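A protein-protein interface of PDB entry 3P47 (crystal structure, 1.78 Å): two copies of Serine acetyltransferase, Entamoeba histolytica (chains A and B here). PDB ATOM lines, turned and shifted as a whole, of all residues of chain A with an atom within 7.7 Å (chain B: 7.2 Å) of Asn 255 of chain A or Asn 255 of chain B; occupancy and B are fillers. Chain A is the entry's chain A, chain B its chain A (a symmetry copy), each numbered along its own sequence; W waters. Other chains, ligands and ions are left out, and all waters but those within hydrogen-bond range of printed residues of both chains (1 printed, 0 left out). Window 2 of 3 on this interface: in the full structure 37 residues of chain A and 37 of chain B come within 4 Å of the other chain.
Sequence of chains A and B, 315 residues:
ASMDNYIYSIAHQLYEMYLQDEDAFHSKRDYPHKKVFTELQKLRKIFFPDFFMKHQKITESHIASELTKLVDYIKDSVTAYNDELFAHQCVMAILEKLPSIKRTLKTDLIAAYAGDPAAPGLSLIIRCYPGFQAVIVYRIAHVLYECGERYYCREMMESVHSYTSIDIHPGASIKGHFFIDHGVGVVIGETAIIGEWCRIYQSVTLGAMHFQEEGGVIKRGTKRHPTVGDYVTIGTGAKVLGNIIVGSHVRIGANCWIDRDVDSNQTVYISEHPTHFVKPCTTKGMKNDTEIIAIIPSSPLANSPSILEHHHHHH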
ATOM      1  N   GLN A 202      24.908  29.635 -23.612  1.00  0.00           N
ATOM      2  CA  GLN A 202      25.005  28.178 -23.651  1.00  0.00           C
ATOM      3  C   GLN A 202      23.643  27.495 -23.404  1.00  0.00           C
ATOM      4  O   GLN A 202      22.774  28.039 -22.698  1.00  0.00           O
ATOM      5  CB  GLN A 202      26.043  27.738 -22.590  1.00  0.00           C
ATOM      6  CG  GLN A 202      25.668  28.108 -21.144  1.00  0.00           C
ATOM      7  CD  GLN A 202      26.276  29.435 -20.680  1.00  0.00           C
ATOM      8  OE1 GLN A 202      26.393  30.367 -21.443  1.00  0.00           O
ATOM      9  NE2 GLN A 202      26.640  29.506 -19.409  1.00  0.00           N
ATOM     10  N   SER A 203      23.442  26.328 -24.018  1.00  0.00           N
ATOM     11  CA  SER A 203      22.242  25.515 -23.777  1.00  0.00           C
ATOM     12  C   SER A 203      20.924  26.169 -24.132  1.00  0.00           C
ATOM     13  O   SER A 203      19.895  25.728 -23.642  1.00  0.00           O
ATOM     14  CB  SER A 203      22.180  25.039 -22.296  1.00  0.00           C
ATOM     15  OG  SER A 203      23.180  24.047 -22.079  1.00  0.00           O
ATOM     16  N   VAL A 204      20.943  27.174 -25.003  1.00  0.00           N
ATOM     17  CA  VAL A 204      19.700  27.776 -25.492  1.00  0.00           C
ATOM     18  C   VAL A 204      19.187  27.035 -26.734  1.00  0.00           C
ATOM     19  O   VAL A 204      19.947  26.765 -27.675  1.00  0.00           O
ATOM     20  CB  VAL A 204      19.904  29.274 -25.820  1.00  0.00           C
ATOM     21  CG1 VAL A 204      18.806  29.802 -26.734  1.00  0.00           C
ATOM     22  CG2 VAL A 204      20.005  30.114 -24.552  1.00  0.00           C
ATOM     23  N   GLY A 235      18.770  33.751 -21.932  1.00  0.00           N
ATOM     24  CA  GLY A 235      19.598  33.242 -20.848  1.00  0.00           C
ATOM     25  C   GLY A 235      19.947  31.773 -20.942  1.00  0.00           C
ATOM     26  O   GLY A 235      19.281  31.003 -21.637  1.00  0.00           O
ATOM     27  N   THR A 236      21.013  31.417 -20.246  1.00  0.00           N
ATOM     28  CA  THR A 236      21.535  30.029 -20.177  1.00  0.00           C
ATOM     29  C   THR A 236      20.419  28.994 -19.965  1.00  0.00           C
ATOM     30  O   THR A 236      19.655  29.082 -18.982  1.00  0.00           O
ATOM     31  CB  THR A 236      22.582  29.924 -18.992  1.00  0.00           C
ATOM     32  OG1 THR A 236      21.915  30.086 -17.730  1.00  0.00           O
ATOM     33  CG2 THR A 236      23.637  31.020 -19.085  1.00  0.00           C
ATOM     34  N   GLY A 237      20.280  28.029 -20.883  1.00  0.00           N
ATOM     35  CA  GLY A 237      19.341  26.920 -20.624  1.00  0.00           C
ATOM     36  C   GLY A 237      17.914  27.099 -21.076  1.00  0.00           C
ATOM     37  O   GLY A 237      17.115  26.143 -21.058  1.00  0.00           O
ATOM     38  N   ALA A 238      17.588  28.312 -21.511  1.00  0.00           N
ATOM     39  CA  ALA A 238      16.245  28.620 -21.995  1.00  0.00           C
ATOM     40  C   ALA A 238      15.890  27.778 -23.229  1.00  0.00           C
ATOM     41  O   ALA A 238      16.701  27.644 -24.175  1.00  0.00           O
ATOM     42  CB  ALA A 238      16.113  30.100 -22.300  1.00  0.00           C
ATOM     43  N   LYS A 239      14.677  27.228 -23.230  1.00  0.00           N
ATOM     44  CA  LYS A 239      14.184  26.425 -24.345  1.00  0.00           C
ATOM     45  C   LYS A 239      12.987  27.139 -24.942  1.00  0.00           C
ATOM     46  O   LYS A 239      11.877  27.143 -24.333  1.00  0.00           O
ATOM     47  CB  LYS A 239      13.728  25.029 -23.874  1.00  0.00           C
ATOM     48  CG  LYS A 239      14.752  24.177 -23.074  1.00  0.00           C
ATOM     49  CD  LYS A 239      15.972  23.919 -23.923  1.00  0.00           C
ATOM     50  CE  LYS A 239      17.006  23.038 -23.223  1.00  0.00           C
ATOM     51  NZ  LYS A 239      17.630  23.725 -22.072  1.00  0.00           N
ATOM     52  N   ILE A 252      15.076  36.858 -21.665  1.00  0.00           N
ATOM     53  CA  ILE A 252      14.614  35.562 -21.178  1.00  0.00           C
ATOM     54  C   ILE A 252      15.580  35.016 -20.115  1.00  0.00           C
ATOM     55  O   ILE A 252      16.802  34.985 -20.342  1.00  0.00           O
ATOM     56  CB  ILE A 252      14.453  34.582 -22.361  1.00  0.00           C
ATOM     57  CG1 ILE A 252      13.457  35.181 -23.372  1.00  0.00           C
ATOM     58  CG2 ILE A 252      14.004  33.191 -21.861  1.00  0.00           C
ATOM     59  CD1 ILE A 252      13.426  34.507 -24.742  1.00  0.00           C
ATOM     60  N   GLY A 253      15.022  34.622 -18.961  1.00  0.00           N
ATOM     61  CA  GLY A 253      15.795  34.010 -17.833  1.00  0.00           C
ATOM     62  C   GLY A 253      16.297  32.565 -17.946  1.00  0.00           C
ATOM     63  O   GLY A 253      15.817  31.746 -18.774  1.00  0.00           O
ATOM     64  N   ALA A 254      17.264  32.223 -17.090  1.00  0.00           N
ATOM     65  CA  ALA A 254      17.867  30.873 -17.126  1.00  0.00           C
ATOM     66  C   ALA A 254      16.818  29.755 -17.015  1.00  0.00           C
ATOM     67  O   ALA A 254      15.858  29.860 -16.254  1.00  0.00           O
ATOM     68  CB  ALA A 254      18.946  30.717 -16.053  1.00  0.00           C
ATOM     69  N   ASN A 255      17.000  28.707 -17.809  1.00  0.00           N
ATOM     70  CA  ASN A 255      16.208  27.495 -17.707  1.00  0.00           C
ATOM     71  C   ASN A 255      14.721  27.659 -18.060  1.00  0.00           C
ATOM     72  O   ASN A 255      13.942  26.739 -17.872  1.00  0.00           O
ATOM     73  CB  ASN A 255      16.398  26.828 -16.328  1.00  0.00           C
ATOM     74  CG  ASN A 255      17.681  26.008 -16.251  1.00  0.00           C
ATOM     75  OD1 ASN A 255      18.458  25.935 -17.215  1.00  0.00           O
ATOM     76  ND2 ASN A 255      17.927  25.408 -15.094  1.00  0.00           N
ATOM     77  N   CYS A 256      14.345  28.800 -18.615  1.00  0.00           N
ATOM     78  CA  CYS A 256      12.939  29.042 -18.985  1.00  0.00           C
ATOM     79  C   CYS A 256      12.430  28.107 -20.083  1.00  0.00           C
ATOM     80  O   CYS A 256      13.128  27.829 -21.018  1.00  0.00           O
ATOM     81  CB  CYS A 256      12.756  30.476 -19.455  1.00  0.00           C
ATOM     82  SG  CYS A 256      12.660  31.672 -18.125  1.00  0.00           S
ATOM     83  N   TRP A 257      11.190  27.665 -19.972  1.00  0.00           N
ATOM     84  CA  TRP A 257      10.559  26.873 -21.007  1.00  0.00           C
ATOM     85  C   TRP A 257       9.499  27.757 -21.679  1.00  0.00           C
ATOM     86  O   TRP A 257       8.445  28.008 -21.091  1.00  0.00           O
ATOM     87  CB  TRP A 257       9.965  25.662 -20.300  1.00  0.00           C
ATOM     88  CG  TRP A 257       8.891  24.874 -20.928  1.00  0.00           C
ATOM     89  CD1 TRP A 257       7.857  24.243 -20.261  1.00  0.00           C
ATOM     90  CD2 TRP A 257       8.731  24.559 -22.302  1.00  0.00           C
ATOM     91  NE1 TRP A 257       7.076  23.570 -21.144  1.00  0.00           N
ATOM     92  CE2 TRP A 257       7.579  23.752 -22.407  1.00  0.00           C
ATOM     93  CE3 TRP A 257       9.440  24.882 -23.458  1.00  0.00           C
ATOM     94  CZ2 TRP A 257       7.122  23.266 -23.618  1.00  0.00           C
ATOM     95  CZ3 TRP A 257       8.978  24.409 -24.659  1.00  0.00           C
ATOM     96  CH2 TRP A 257       7.832  23.599 -24.732  1.00  0.00           C
ATOM     97  N   ILE A 258       9.799  28.238 -22.887  1.00  0.00           N
ATOM     98  CA  ILE A 258       8.941  29.205 -23.589  1.00  0.00           C
ATOM     99  C   ILE A 258       8.243  28.538 -24.782  1.00  0.00           C
ATOM    100  O   ILE A 258       8.895  28.052 -25.694  1.00  0.00           O
ATOM    101  CB  ILE A 258       9.738  30.477 -24.037  1.00  0.00           C
ATOM    102  CG1 ILE A 258      10.436  31.175 -22.848  1.00  0.00           C
ATOM    103  CG2 ILE A 258       8.843  31.459 -24.777  1.00  0.00           C
ATOM    104  CD1 ILE A 258       9.596  31.379 -21.601  1.00  0.00           C
ATOM    105  N   ILE A 270      10.985  33.002 -13.631  1.00  0.00           N
ATOM    106  CA  ILE A 270       9.994  32.357 -12.750  1.00  0.00           C
ATOM    107  C   ILE A 270      10.460  32.383 -11.292  1.00  0.00           C
ATOM    108  O   ILE A 270      10.113  33.293 -10.530  1.00  0.00           O
ATOM    109  CB  ILE A 270       9.625  30.898 -13.193  1.00  0.00           C
ATOM    110  CG1 ILE A 270       9.096  30.876 -14.635  1.00  0.00           C
ATOM    111  CG2 ILE A 270       8.578  30.298 -12.245  1.00  0.00           C
ATOM    112  CD1 ILE A 270       9.079  29.508 -15.296  1.00  0.00           C
ATOM    113  N   SER B 203      26.127  20.221 -18.100  1.00  0.00           N
ATOM    114  CA  SER B 203      25.225  21.373 -18.217  1.00  0.00           C
ATOM    115  C   SER B 203      25.155  22.280 -17.007  1.00  0.00           C
ATOM    116  O   SER B 203      24.194  23.024 -16.882  1.00  0.00           O
ATOM    117  CB  SER B 203      23.781  20.916 -18.583  1.00  0.00           C
ATOM    118  OG  SER B 203      23.758  20.463 -19.934  1.00  0.00           O
ATOM    119  N   MET B 209      25.130  35.992 -16.697  1.00  0.00           N
ATOM    120  CA  MET B 209      24.407  36.397 -17.898  1.00  0.00           C
ATOM    121  C   MET B 209      24.337  37.919 -17.919  1.00  0.00           C
ATOM    122  O   MET B 209      24.195  38.537 -16.874  1.00  0.00           O
ATOM    123  CB  MET B 209      22.974  35.952 -17.786  1.00  0.00           C
ATOM    124  CG  MET B 209      22.708  34.511 -17.789  1.00  0.00           C
ATOM    125  SD  MET B 209      20.934  34.442 -18.020  1.00  0.00           S
ATOM    126  CE  MET B 209      20.262  35.168 -16.515  1.00  0.00           C
ATOM    127  N   GLY B 235      24.190  19.669  -9.312  1.00  0.00           N
ATOM    128  CA  GLY B 235      23.454  18.731 -10.146  1.00  0.00           C
ATOM    129  C   GLY B 235      23.321  19.130 -11.599  1.00  0.00           C
ATOM    130  O   GLY B 235      23.470  20.301 -11.954  1.00  0.00           O
ATOM    131  N   THR B 236      23.059  18.128 -12.422  1.00  0.00           N
ATOM    132  CA  THR B 236      22.874  18.283 -13.886  1.00  0.00           C
ATOM    133  C   THR B 236      21.977  19.479 -14.239  1.00  0.00           C
ATOM    134  O   THR B 236      20.821  19.560 -13.776  1.00  0.00           O
ATOM    135  CB  THR B 236      22.237  16.956 -14.474  1.00  0.00           C
ATOM    136  OG1 THR B 236      20.894  16.799 -13.988  1.00  0.00           O
ATOM    137  CG2 THR B 236      23.020  15.724 -14.035  1.00  0.00           C
ATOM    138  N   GLY B 237      22.490  20.434 -15.026  1.00  0.00           N
ATOM    139  CA  GLY B 237      21.607  21.504 -15.529  1.00  0.00           C
ATOM    140  C   GLY B 237      21.462  22.741 -14.681  1.00  0.00           C
ATOM    141  O   GLY B 237      20.885  23.753 -15.124  1.00  0.00           O
ATOM    142  N   ALA B 238      22.007  22.685 -13.470  1.00  0.00           N
ATOM    143  CA  ALA B 238      21.956  23.819 -12.550  1.00  0.00           C
ATOM    144  C   ALA B 238      22.688  25.039 -13.128  1.00  0.00           C
ATOM    145  O   ALA B 238      23.820  24.924 -13.655  1.00  0.00           O
ATOM    146  CB  ALA B 238      22.532  23.438 -11.200  1.00  0.00           C
ATOM    147  N   LYS B 239      22.057  26.206 -13.014  1.00  0.00           N
ATOM    148  CA  LYS B 239      22.638  27.459 -13.488  1.00  0.00           C
ATOM    149  C   LYS B 239      22.846  28.362 -12.288  1.00  0.00           C
ATOM    150  O   LYS B 239      21.856  28.922 -11.733  1.00  0.00           O
ATOM    151  CB  LYS B 239      21.696  28.176 -14.476  1.00  0.00           C
ATOM    152  CG  LYS B 239      21.205  27.368 -15.709  1.00  0.00           C
ATOM    153  CD  LYS B 239      22.388  26.945 -16.543  1.00  0.00           C
ATOM    154  CE  LYS B 239      21.983  26.188 -17.807  1.00  0.00           C
ATOM    155  NZ  LYS B 239      21.396  24.867 -17.497  1.00  0.00           N
ATOM    156  N   ILE B 252      23.199  21.066  -4.791  1.00  0.00           N
ATOM    157  CA  ILE B 252      22.265  21.739  -5.688  1.00  0.00           C
ATOM    158  C   ILE B 252      21.594  20.720  -6.622  1.00  0.00           C
ATOM    159  O   ILE B 252      22.287  19.900  -7.251  1.00  0.00           O
ATOM    160  CB  ILE B 252      22.998  22.843  -6.481  1.00  0.00           C
ATOM    161  CG1 ILE B 252      23.625  23.838  -5.484  1.00  0.00           C
ATOM    162  CG2 ILE B 252      22.035  23.541  -7.467  1.00  0.00           C
ATOM    163  CD1 ILE B 252      24.650  24.802  -6.076  1.00  0.00           C
ATOM    164  N   GLY B 253      20.255  20.765  -6.678  1.00  0.00           N
ATOM    165  CA  GLY B 253      19.431  19.891  -7.574  1.00  0.00           C
ATOM    166  C   GLY B 253      19.384  20.172  -9.080  1.00  0.00           C
ATOM    167  O   GLY B 253      19.715  21.283  -9.571  1.00  0.00           O
ATOM    168  N   ALA B 254      18.945  19.164  -9.840  1.00  0.00           N
ATOM    169  CA  ALA B 254      18.895  19.291 -11.312  1.00  0.00           C
ATOM    170  C   ALA B 254      18.093  20.518 -11.772  1.00  0.00           C
ATOM    171  O   ALA B 254      17.056  20.850 -11.201  1.00  0.00           O
ATOM    172  CB  ALA B 254      18.357  18.015 -11.962  1.00  0.00           C
ATOM    173  N   ASN B 255      18.610  21.203 -12.786  1.00  0.00           N
ATOM    174  CA  ASN B 255      17.899  22.278 -13.454  1.00  0.00           C
ATOM    175  C   ASN B 255      17.639  23.522 -12.588  1.00  0.00           C
ATOM    176  O   ASN B 255      16.929  24.421 -13.007  1.00  0.00           O
ATOM    177  CB  ASN B 255      16.602  21.756 -14.109  1.00  0.00           C
ATOM    178  CG  ASN B 255      16.861  21.080 -15.451  1.00  0.00           C
ATOM    179  OD1 ASN B 255      18.008  20.973 -15.909  1.00  0.00           O
ATOM    180  ND2 ASN B 255      15.798  20.592 -16.079  1.00  0.00           N
ATOM    181  N   CYS B 256      18.251  23.592 -11.417  1.00  0.00           N
ATOM    182  CA  CYS B 256      18.057  24.747 -10.523  1.00  0.00           C
ATOM    183  C   CYS B 256      18.585  26.060 -11.104  1.00  0.00           C
ATOM    184  O   CYS B 256      19.625  26.086 -11.701  1.00  0.00           O
ATOM    185  CB  CYS B 256      18.746  24.504  -9.190  1.00  0.00           C
ATOM    186  SG  CYS B 256      17.830  23.435  -8.082  1.00  0.00           S
ATOM    187  N   TRP B 257      17.870  27.148 -10.882  1.00  0.00           N
ATOM    188  CA  TRP B 257      18.328  28.463 -11.277  1.00  0.00           C
ATOM    189  C   TRP B 257      18.698  29.225  -9.998  1.00  0.00           C
ATOM    190  O   TRP B 257      17.810  29.649  -9.254  1.00  0.00           O
ATOM    191  CB  TRP B 257      17.167  29.096 -12.033  1.00  0.00           C
ATOM    192  CG  TRP B 257      17.085  30.558 -12.203  1.00  0.00           C
ATOM    193  CD1 TRP B 257      15.920  31.303 -12.238  1.00  0.00           C
ATOM    194  CD2 TRP B 257      18.150  31.470 -12.418  1.00  0.00           C
ATOM    195  NE1 TRP B 257      16.211  32.610 -12.455  1.00  0.00           N
ATOM    196  CE2 TRP B 257      17.571  32.749 -12.560  1.00  0.00           C
ATOM    197  CE3 TRP B 257      19.535  31.339 -12.500  1.00  0.00           C
ATOM    198  CZ2 TRP B 257      18.329  33.884 -12.777  1.00  0.00           C
ATOM    199  CZ3 TRP B 257      20.284  32.470 -12.703  1.00  0.00           C
ATOM    200  CH2 TRP B 257      19.680  33.729 -12.849  1.00  0.00           C
ATOM    201  N   ILE B 258      20.001  29.367  -9.741  1.00  0.00           N
ATOM    202  CA  ILE B 258      20.501  29.952  -8.488  1.00  0.00           C
ATOM    203  C   ILE B 258      21.099  31.341  -8.745  1.00  0.00           C
ATOM    204  O   ILE B 258      22.050  31.481  -9.500  1.00  0.00           O
ATOM    205  CB  ILE B 258      21.532  29.013  -7.776  1.00  0.00           C
ATOM    206  CG1 ILE B 258      20.946  27.612  -7.491  1.00  0.00           C
ATOM    207  CG2 ILE B 258      22.056  29.639  -6.491  1.00  0.00           C
ATOM    208  CD1 ILE B 258      19.555  27.576  -6.885  1.00  0.00           C
ATOM    209  N   ILE B 270      13.520  22.014  -6.039  1.00  0.00           N
ATOM    210  CA  ILE B 270      12.181  22.629  -6.105  1.00  0.00           C
ATOM    211  C   ILE B 270      11.098  21.563  -6.291  1.00  0.00           C
ATOM    212  O   ILE B 270      10.508  21.079  -5.316  1.00  0.00           O
ATOM    213  CB  ILE B 270      12.062  23.744  -7.202  1.00  0.00           C
ATOM    214  CG1 ILE B 270      13.107  24.849  -6.983  1.00  0.00           C
ATOM    215  CG2 ILE B 270      10.654  24.351  -7.200  1.00  0.00           C
ATOM    216  CD1 ILE B 270      13.345  25.758  -8.177  1.00  0.00           C
HETATM  217  O   HOH W   1      24.568  21.144 -23.159  1.00  0.00           O
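Among the printed residues, pairs that only touch across the chains: Gly 235 of chain A with Met 209 of chain B (3.3 Å), Thr 236 of chain A with Lys 239 of chain B (3.4 Å), Ala 254 of chain A with Trp 257 of chain B (3.7 Å), Asn 255 of chain A with Cys 256 of chain B (3.9 Å) and Gly 237 of chain A with Lys 239 of chain B (3.9 Å).
The backbone NH (N) of Thr 236 of chain A lies within hydrogen-bond range of the side-chain sulfur (SD) of Met 209 of chain B (3.8 Å).
The backbone carbonyl oxygen (O) of Gly 237 of chain B is in hydrogen-bond range of the side-chain amide nitrogen (ND2) of Asn 255 of chain A, at 3.4 Å.
OD1 of Asn 255 of chain A lies within hydrogen-bond range of NZ of Lys 239 of chain B, at 3.1 Å.
ND2 of Asn 255 of chain A sits at hydrogen-bond distance from O of Asn 255 of chain B, at 2.5 Å.
The backbone carbonyl oxygen (O) of Gln 202 of chain A sits at hydrogen-bond distance from the backbone NH (N) of Gly 237 of chain A (3.1 Å).
The backbone NH (N) of Gly 235 of chain A sits at hydrogen-bond distance from the backbone carbonyl oxygen (O) of Ile 252 of chain A, 2.8 Å away.
O of Ser 203 of chain B sits at hydrogen-bond distance from NZ of Lys 239 of chain B (3.4 Å).
The backbone carbonyl oxygen (O) of Thr 236 of chain B sits at hydrogen-bond distance from the backbone NH (N) of Asn 255 of chain B.
The backbone NH (N) of Lys 239 of chain B lies within hydrogen-bond range of the backbone carbonyl oxygen (O) of Cys 256 of chain B (2.8 Å).
O of Gly 253 of chain B lies within hydrogen-bond range of SG of Cys 256 of chain B (3.2 Å).
Water W1 lies within hydrogen-bond range of the side-chain hydroxyl (OG) of Ser 203 of chain A (3.4 Å) and the side-chain hydroxyl (OG) of Ser 203 of chain B (3.4 Å).
Of the 16 printed residues of chain A, 5 touch a printed residue of chain B.
Hydrophobic or aromatic side chains of chain A that line the printed part of chain B: Ala 254.
Of the 15 printed residues of chain B, 6 touch a printed residue of chain A.
Hydrophobic or aromatic side chains of chain B that line the printed part of chain A: Met 209 and Trp 257.
Among the printed residues, 9 pairs touch across the chains.
Of the printed residues of chain B, Gly 235 of chain A touches Met 209 (3.3 Å).
Of the printed residues of chain B, Thr 236 of chain A touches Met 209 (3.8 Å) and Lys 239 (3.4 Å).
Of the printed residues of chain B, Gly 237 of chain A touches Lys 239.
No residue of chain A comes within 4 Å of Ala 254 of chain B.
Printed residues of chain A within 4 Å of Asn 255 of chain B: Asn 255.
Of the printed residues of chain A, Cys 256 of chain B touches Asn 255.
Printed residues of chain A within 4 Å of Trp 257 of chain B: Ala 254 (3.7 Å).
The nearest residue of chain B that does not touch Asn 255 of chain A is Trp 257 of chain B (4.6 Å).
The nearest residue of chain A that does not touch Asn 255 of chain B is Ala 254 of chain A (6.4 Å).
Thr 236 of chain A touches Lys 239 of chain B, but with the chains exchanged Lys 239 of chain A does not touch Thr 236 of chain B (9.8 Å).
Asn 255 of chain A touches Gly 237 of chain B, but with the chains exchanged Gly 237 of chain A does not touch Asn 255 of chain B (7.4 Å).
Asn 255 of chain A touches Lys 239 of chain B, but with the chains exchanged Lys 239 of chain A does not touch Asn 255 of chain B (6.8 Å).
Asn 255 of chain B touches its own counterpart, Asn 255 of chain A.
Positions printed for both chains: 203, 235, 236, 237, 238, 239, 252, 253, 254, 255, 256, 257, 258 and 270.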
